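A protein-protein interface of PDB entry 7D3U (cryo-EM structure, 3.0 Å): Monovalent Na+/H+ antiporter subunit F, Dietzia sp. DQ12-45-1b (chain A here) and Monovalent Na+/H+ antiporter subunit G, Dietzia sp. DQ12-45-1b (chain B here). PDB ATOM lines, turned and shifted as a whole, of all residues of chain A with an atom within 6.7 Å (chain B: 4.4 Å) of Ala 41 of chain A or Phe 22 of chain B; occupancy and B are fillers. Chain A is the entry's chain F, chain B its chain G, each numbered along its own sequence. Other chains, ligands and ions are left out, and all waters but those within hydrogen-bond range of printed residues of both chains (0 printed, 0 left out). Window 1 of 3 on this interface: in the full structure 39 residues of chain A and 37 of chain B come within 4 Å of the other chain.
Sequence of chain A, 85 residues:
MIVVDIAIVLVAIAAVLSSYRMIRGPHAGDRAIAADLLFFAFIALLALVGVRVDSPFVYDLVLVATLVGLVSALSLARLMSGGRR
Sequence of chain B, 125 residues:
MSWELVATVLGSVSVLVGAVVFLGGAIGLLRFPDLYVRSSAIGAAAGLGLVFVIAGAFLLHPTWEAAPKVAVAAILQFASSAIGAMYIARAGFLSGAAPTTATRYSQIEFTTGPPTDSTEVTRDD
Among the printed residues, pairs that only touch across the chains: Phe 40 of chain A with Ala 46 of chain B (3.1 Å), Ala 14 of chain A with Ala 26 of chain B (3.2 Å), Phe 40 of chain A with Leu 50 of chain B (3.4 Å), Ala 41 of chain A with Phe 22 of chain B (3.4 Å), Phe 40 of chain A with Phe 22 of chain B (3.4 Å), Ala 44 of chain A with Leu 50 of chain B (3.4 Å), Ala 14 of chain A with Phe 22 of chain B (3.5 Å), Ala 14 of chain A with Leu 23 of chain B (3.6 Å), Ile 43 of chain A with Leu 50 of chain B (3.7 Å), Leu 37 of chain A with Ala 46 of chain B (3.7 Å), Ala 44 of chain A with Phe 22 of chain B (3.8 Å), Leu 10 of chain A with Ala 19 of chain B (3.8 Å), Leu 10 of chain A with Leu 23 of chain B (3.8 Å), Leu 37 of chain A with Phe 22 of chain B (3.9 Å) and Val 11 of chain A with Ala 19 of chain B (3.9 Å).
Of the printed residues of chain B, Val 11 of chain A touches Ala 19. Of chain B, only Phe 22 (3.4 Å) comes within 4 Å of Ala 41 of chain A. Of the printed residues of chain A, Ala 19 of chain B touches Leu 10 (3.8 Å) and Val 11 (3.9 Å). Phe 22 of chain B touches five residues of chain A. Printed residues of chain A within 4 Å of Ala 46 of chain B: Leu 37 and Phe 40.
Printed residues of chain A that touch a printed residue of chain B: Leu 10, Val 11, Ala 14, Leu 37, Phe 40, Ala 41, Ile 43 and Ala 44. Along chain A the printed residues that touch a printed residue of chain B span positions 10 to 44. Of the 12 printed residues of chain B, 6 touch a printed residue of chain A. Printed residues of chain B that touch a printed residue of chain A: Ala 19, Phe 22, Leu 23, Ala 26, Ala 46 and Leu 50. Among the printed residues, no Asp or Glu carboxylate lies within 4 Å of a Lys or Arg side-chain nitrogen of the other chain.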
ATOM      1  N   LEU A  10     -14.656  16.145   7.125  1.00  0.00           N
ATOM      2  CA  LEU A  10     -14.216  15.647   8.425  1.00  0.00           C
ATOM      3  C   LEU A  10     -14.734  14.237   8.685  1.00  0.00           C
ATOM      4  O   LEU A  10     -13.991  13.376   9.170  1.00  0.00           O
ATOM      5  CB  LEU A  10     -14.666  16.599   9.531  1.00  0.00           C
ATOM      6  CG  LEU A  10     -13.893  17.914   9.621  1.00  0.00           C
ATOM      7  CD1 LEU A  10     -14.339  18.717  10.830  1.00  0.00           C
ATOM      8  CD2 LEU A  10     -12.397  17.653   9.667  1.00  0.00           C
ATOM      9  N   VAL A  11     -16.003  13.976   8.360  1.00  0.00           N
ATOM     10  CA  VAL A  11     -16.548  12.634   8.536  1.00  0.00           C
ATOM     11  C   VAL A  11     -15.865  11.648   7.600  1.00  0.00           C
ATOM     12  O   VAL A  11     -15.631  10.494   7.972  1.00  0.00           O
ATOM     13  CB  VAL A  11     -18.075  12.642   8.335  1.00  0.00           C
ATOM     14  CG1 VAL A  11     -18.620  11.230   8.349  1.00  0.00           C
ATOM     15  CG2 VAL A  11     -18.741  13.463   9.419  1.00  0.00           C
ATOM     16  N   ALA A  12     -15.506  12.079   6.390  1.00  0.00           N
ATOM     17  CA  ALA A  12     -14.794  11.194   5.473  1.00  0.00           C
ATOM     18  C   ALA A  12     -13.401  10.863   5.993  1.00  0.00           C
ATOM     19  O   ALA A  12     -12.952   9.717   5.892  1.00  0.00           O
ATOM     20  CB  ALA A  12     -14.715  11.828   4.087  1.00  0.00           C
ATOM     21  N   ALA A  14     -12.517  10.853   9.162  1.00  0.00           N
ATOM     22  CA  ALA A  14     -12.745   9.948  10.283  1.00  0.00           C
ATOM     23  C   ALA A  14     -13.029   8.533   9.797  1.00  0.00           C
ATOM     24  O   ALA A  14     -12.526   7.557  10.365  1.00  0.00           O
ATOM     25  CB  ALA A  14     -13.900  10.459  11.141  1.00  0.00           C
ATOM     26  N   ALA A  15     -13.830   8.407   8.739  1.00  0.00           N
ATOM     27  CA  ALA A  15     -14.135   7.095   8.186  1.00  0.00           C
ATOM     28  C   ALA A  15     -12.886   6.431   7.627  1.00  0.00           C
ATOM     29  O   ALA A  15     -12.699   5.221   7.780  1.00  0.00           O
ATOM     30  CB  ALA A  15     -15.206   7.226   7.106  1.00  0.00           C
ATOM     31  N   ASP A  36     -18.685  -0.788  13.034  1.00  0.00           N
ATOM     32  CA  ASP A  36     -19.776  -0.064  13.681  1.00  0.00           C
ATOM     33  C   ASP A  36     -19.592   1.443  13.540  1.00  0.00           C
ATOM     34  O   ASP A  36     -20.511   2.162  13.114  1.00  0.00           O
ATOM     35  CB  ASP A  36     -19.859  -0.466  15.153  1.00  0.00           C
ATOM     36  CG  ASP A  36     -20.851   0.371  15.930  1.00  0.00           C
ATOM     37  OD1 ASP A  36     -22.055   0.039  15.911  1.00  0.00           O
ATOM     38  OD2 ASP A  36     -20.427   1.360  16.563  1.00  0.00           O
ATOM     39  N   LEU A  37     -18.407   1.943  13.906  1.00  0.00           N
ATOM     40  CA  LEU A  37     -18.135   3.368  13.759  1.00  0.00           C
ATOM     41  C   LEU A  37     -18.304   3.816  12.315  1.00  0.00           C
ATOM     42  O   LEU A  37     -18.790   4.923  12.062  1.00  0.00           O
ATOM     43  CB  LEU A  37     -16.726   3.689  14.261  1.00  0.00           C
ATOM     44  CG  LEU A  37     -16.334   5.157  14.460  1.00  0.00           C
ATOM     45  CD1 LEU A  37     -15.801   5.789  13.185  1.00  0.00           C
ATOM     46  CD2 LEU A  37     -17.510   5.951  14.997  1.00  0.00           C
ATOM     47  N   LEU A  38     -17.944   2.963  11.355  1.00  0.00           N
ATOM     48  CA  LEU A  38     -18.059   3.343   9.954  1.00  0.00           C
ATOM     49  C   LEU A  38     -19.507   3.338   9.488  1.00  0.00           C
ATOM     50  O   LEU A  38     -19.893   4.169   8.666  1.00  0.00           O
ATOM     51  CB  LEU A  38     -17.202   2.421   9.093  1.00  0.00           C
ATOM     52  CG  LEU A  38     -15.715   2.576   9.394  1.00  0.00           C
ATOM     53  CD1 LEU A  38     -14.886   1.561   8.646  1.00  0.00           C
ATOM     54  CD2 LEU A  38     -15.289   3.974   9.018  1.00  0.00           C
ATOM     55  N   PHE A  39     -20.326   2.416   9.993  1.00  0.00           N
ATOM     56  CA  PHE A  39     -21.750   2.463   9.672  1.00  0.00           C
ATOM     57  C   PHE A  39     -22.372   3.753  10.184  1.00  0.00           C
ATOM     58  O   PHE A  39     -23.172   4.393   9.486  1.00  0.00           O
ATOM     59  CB  PHE A  39     -22.475   1.254  10.263  1.00  0.00           C
ATOM     60  CG  PHE A  39     -21.976  -0.065   9.754  1.00  0.00           C
ATOM     61  CD1 PHE A  39     -21.427  -0.175   8.491  1.00  0.00           C
ATOM     62  CD2 PHE A  39     -22.058  -1.198  10.544  1.00  0.00           C
ATOM     63  CE1 PHE A  39     -20.967  -1.390   8.025  1.00  0.00           C
ATOM     64  CE2 PHE A  39     -21.598  -2.414  10.083  1.00  0.00           C
ATOM     65  CZ  PHE A  39     -21.053  -2.510   8.823  1.00  0.00           C
ATOM     66  N   PHE A  40     -21.999   4.167  11.394  1.00  0.00           N
ATOM     67  CA  PHE A  40     -22.555   5.408  11.923  1.00  0.00           C
ATOM     68  C   PHE A  40     -22.033   6.619  11.150  1.00  0.00           C
ATOM     69  O   PHE A  40     -22.784   7.569  10.884  1.00  0.00           O
ATOM     70  CB  PHE A  40     -22.254   5.518  13.417  1.00  0.00           C
ATOM     71  CG  PHE A  40     -23.151   4.664  14.271  1.00  0.00           C
ATOM     72  CD1 PHE A  40     -23.021   3.289  14.275  1.00  0.00           C
ATOM     73  CD2 PHE A  40     -24.127   5.234  15.064  1.00  0.00           C
ATOM     74  CE1 PHE A  40     -23.843   2.502  15.050  1.00  0.00           C
ATOM     75  CE2 PHE A  40     -24.952   4.453  15.840  1.00  0.00           C
ATOM     76  CZ  PHE A  40     -24.808   3.085  15.834  1.00  0.00           C
ATOM     77  N   ALA A  41     -20.761   6.590  10.749  1.00  0.00           N
ATOM     78  CA  ALA A  41     -20.232   7.657   9.906  1.00  0.00           C
ATOM     79  C   ALA A  41     -20.917   7.688   8.546  1.00  0.00           C
ATOM     80  O   ALA A  41     -21.095   8.762   7.966  1.00  0.00           O
ATOM     81  CB  ALA A  41     -18.723   7.496   9.737  1.00  0.00           C
ATOM     82  N   PHE A  42     -21.321   6.527   8.026  1.00  0.00           N
ATOM     83  CA  PHE A  42     -22.032   6.495   6.756  1.00  0.00           C
ATOM     84  C   PHE A  42     -23.440   7.050   6.891  1.00  0.00           C
ATOM     85  O   PHE A  42     -23.940   7.692   5.964  1.00  0.00           O
ATOM     86  CB  PHE A  42     -22.076   5.072   6.205  1.00  0.00           C
ATOM     87  CG  PHE A  42     -20.931   4.742   5.295  1.00  0.00           C
ATOM     88  CD1 PHE A  42     -20.825   5.342   4.058  1.00  0.00           C
ATOM     89  CD2 PHE A  42     -19.968   3.826   5.672  1.00  0.00           C
ATOM     90  CE1 PHE A  42     -19.777   5.041   3.216  1.00  0.00           C
ATOM     91  CE2 PHE A  42     -18.918   3.523   4.837  1.00  0.00           C
ATOM     92  CZ  PHE A  42     -18.822   4.131   3.607  1.00  0.00           C
ATOM     93  N   ILE A  43     -24.096   6.817   8.028  1.00  0.00           N
ATOM     94  CA  ILE A  43     -25.380   7.474   8.267  1.00  0.00           C
ATOM     95  C   ILE A  43     -25.197   8.987   8.329  1.00  0.00           C
ATOM     96  O   ILE A  43     -25.995   9.755   7.769  1.00  0.00           O
ATOM     97  CB  ILE A  43     -26.034   6.931   9.550  1.00  0.00           C
ATOM     98  CG1 ILE A  43     -26.177   5.415   9.472  1.00  0.00           C
ATOM     99  CG2 ILE A  43     -27.389   7.570   9.763  1.00  0.00           C
ATOM    100  CD1 ILE A  43     -26.778   4.805  10.710  1.00  0.00           C
ATOM    101  N   ALA A  44     -24.139   9.439   9.010  1.00  0.00           N
ATOM    102  CA  ALA A  44     -23.849  10.870   9.050  1.00  0.00           C
ATOM    103  C   ALA A  44     -23.615  11.426   7.652  1.00  0.00           C
ATOM    104  O   ALA A  44     -24.077  12.526   7.324  1.00  0.00           O
ATOM    105  CB  ALA A  44     -22.635  11.136   9.938  1.00  0.00           C
ATOM    106  N   LEU A  45     -22.894  10.678   6.817  1.00  0.00           N
ATOM    107  CA  LEU A  45     -22.640  11.128   5.455  1.00  0.00           C
ATOM    108  C   LEU A  45     -23.920  11.153   4.634  1.00  0.00           C
ATOM    109  O   LEU A  45     -24.103  12.039   3.798  1.00  0.00           O
ATOM    110  CB  LEU A  45     -21.595  10.237   4.789  1.00  0.00           C
ATOM    111  CG  LEU A  45     -20.162  10.746   4.881  1.00  0.00           C
ATOM    112  CD1 LEU A  45     -19.316  10.091   3.819  1.00  0.00           C
ATOM    113  CD2 LEU A  45     -20.124  12.254   4.735  1.00  0.00           C
ATOM    114  N   LEU A  46     -24.812  10.185   4.852  1.00  0.00           N
ATOM    115  CA  LEU A  46     -26.118  10.222   4.203  1.00  0.00           C
ATOM    116  C   LEU A  46     -26.847  11.513   4.539  1.00  0.00           C
ATOM    117  O   LEU A  46     -27.355  12.206   3.649  1.00  0.00           O
ATOM    118  CB  LEU A  46     -26.952   9.014   4.626  1.00  0.00           C
ATOM    119  CG  LEU A  46     -26.737   7.706   3.868  1.00  0.00           C
ATOM    120  CD1 LEU A  46     -27.712   6.648   4.353  1.00  0.00           C
ATOM    121  CD2 LEU A  46     -26.897   7.931   2.381  1.00  0.00           C
ATOM    122  N   GLY B  18     -20.734  17.482  15.521  1.00  0.00           N
ATOM    123  CA  GLY B  18     -20.860  16.060  15.251  1.00  0.00           C
ATOM    124  C   GLY B  18     -19.717  15.515  14.417  1.00  0.00           C
ATOM    125  O   GLY B  18     -19.220  14.415  14.675  1.00  0.00           O
ATOM    126  N   ALA B  19     -19.280  16.271  13.409  1.00  0.00           N
ATOM    127  CA  ALA B  19     -18.141  15.832  12.612  1.00  0.00           C
ATOM    128  C   ALA B  19     -16.872  15.790  13.450  1.00  0.00           C
ATOM    129  O   ALA B  19     -16.061  14.866  13.318  1.00  0.00           O
ATOM    130  CB  ALA B  19     -17.958  16.749  11.405  1.00  0.00           C
ATOM    131  N   VAL B  20     -16.683  16.779  14.327  1.00  0.00           N
ATOM    132  CA  VAL B  20     -15.510  16.781  15.195  1.00  0.00           C
ATOM    133  C   VAL B  20     -15.547  15.585  16.139  1.00  0.00           C
ATOM    134  O   VAL B  20     -14.517  14.956  16.409  1.00  0.00           O
ATOM    135  CB  VAL B  20     -15.420  18.116  15.958  1.00  0.00           C
ATOM    136  CG1 VAL B  20     -14.688  17.941  17.276  1.00  0.00           C
ATOM    137  CG2 VAL B  20     -14.736  19.162  15.094  1.00  0.00           C
ATOM    138  N   VAL B  21     -16.736  15.238  16.638  1.00  0.00           N
ATOM    139  CA  VAL B  21     -16.858  14.087  17.526  1.00  0.00           C
ATOM    140  C   VAL B  21     -16.571  12.795  16.778  1.00  0.00           C
ATOM    141  O   VAL B  21     -15.933  11.882  17.312  1.00  0.00           O
ATOM    142  CB  VAL B  21     -18.250  14.066  18.176  1.00  0.00           C
ATOM    143  CG1 VAL B  21     -18.495  12.742  18.871  1.00  0.00           C
ATOM    144  CG2 VAL B  21     -18.370  15.202  19.151  1.00  0.00           C
ATOM    145  N   PHE B  22     -17.045  12.688  15.535  1.00  0.00           N
ATOM    146  CA  PHE B  22     -16.727  11.515  14.729  1.00  0.00           C
ATOM    147  C   PHE B  22     -15.227  11.403  14.501  1.00  0.00           C
ATOM    148  O   PHE B  22     -14.658  10.309  14.578  1.00  0.00           O
ATOM    149  CB  PHE B  22     -17.465  11.573  13.395  1.00  0.00           C
ATOM    150  CG  PHE B  22     -18.700  10.731  13.354  1.00  0.00           C
ATOM    151  CD1 PHE B  22     -18.610   9.354  13.299  1.00  0.00           C
ATOM    152  CD2 PHE B  22     -19.952  11.315  13.361  1.00  0.00           C
ATOM    153  CE1 PHE B  22     -19.745   8.575  13.264  1.00  0.00           C
ATOM    154  CE2 PHE B  22     -21.090  10.540  13.323  1.00  0.00           C
ATOM    155  CZ  PHE B  22     -20.987   9.169  13.273  1.00  0.00           C
ATOM    156  N   LEU B  23     -14.567  12.531  14.233  1.00  0.00           N
ATOM    157  CA  LEU B  23     -13.120  12.508  14.038  1.00  0.00           C
ATOM    158  C   LEU B  23     -12.398  12.114  15.320  1.00  0.00           C
ATOM    159  O   LEU B  23     -11.394  11.395  15.278  1.00  0.00           O
ATOM    160  CB  LEU B  23     -12.639  13.869  13.540  1.00  0.00           C
ATOM    161  CG  LEU B  23     -11.198  13.956  13.045  1.00  0.00           C
ATOM    162  CD1 LEU B  23     -11.134  14.739  11.749  1.00  0.00           C
ATOM    163  CD2 LEU B  23     -10.320  14.605  14.100  1.00  0.00           C
ATOM    164  N   GLY B  24     -12.903  12.562  16.470  1.00  0.00           N
ATOM    165  CA  GLY B  24     -12.294  12.171  17.730  1.00  0.00           C
ATOM    166  C   GLY B  24     -12.479  10.696  18.028  1.00  0.00           C
ATOM    167  O   GLY B  24     -11.556  10.027  18.499  1.00  0.00           O
ATOM    168  N   GLY B  25     -13.669  10.165  17.745  1.00  0.00           N
ATOM    169  CA  GLY B  25     -13.903   8.746  17.937  1.00  0.00           C
ATOM    170  C   GLY B  25     -13.131   7.885  16.960  1.00  0.00           C
ATOM    171  O   GLY B  25     -12.835   6.724  17.252  1.00  0.00           O
ATOM    172  N   ALA B  26     -12.795   8.435  15.792  1.00  0.00           N
ATOM    173  CA  ALA B  26     -11.960   7.705  14.846  1.00  0.00           C
ATOM    174  C   ALA B  26     -10.496   7.723  15.265  1.00  0.00           C
ATOM    175  O   ALA B  26      -9.819   6.692  15.198  1.00  0.00           O
ATOM    176  CB  ALA B  26     -12.116   8.288  13.447  1.00  0.00           C
ATOM    177  N   ALA B  46     -19.794   7.356  18.367  1.00  0.00           N
ATOM    178  CA  ALA B  46     -20.702   7.029  17.273  1.00  0.00           C
ATOM    179  C   ALA B  46     -22.142   7.405  17.583  1.00  0.00           C
ATOM    180  O   ALA B  46     -22.936   7.585  16.655  1.00  0.00           O
ATOM    181  CB  ALA B  46     -20.615   5.539  16.945  1.00  0.00           C
ATOM    182  N   GLY B  49     -21.898  11.973  18.129  1.00  0.00           N
ATOM    183  CA  GLY B  49     -21.597  12.630  16.869  1.00  0.00           C
ATOM    184  C   GLY B  49     -22.691  12.445  15.837  1.00  0.00           C
ATOM    185  O   GLY B  49     -23.069  13.392  15.143  1.00  0.00           O
ATOM    186  N   LEU B  50     -23.238  11.233  15.742  1.00  0.00           N
ATOM    187  CA  LEU B  50     -24.261  10.981  14.735  1.00  0.00           C
ATOM    188  C   LEU B  50     -25.573  11.672  15.085  1.00  0.00           C
ATOM    189  O   LEU B  50     -26.254  12.195  14.198  1.00  0.00           O
ATOM    190  CB  LEU B  50     -24.472   9.480  14.553  1.00  0.00           C
ATOM    191  CG  LEU B  50     -25.458   9.121  13.442  1.00  0.00           C
ATOM    192  CD1 LEU B  50     -25.185   9.933  12.200  1.00  0.00           C
ATOM    193  CD2 LEU B  50     -25.409   7.647  13.114  1.00  0.00           C
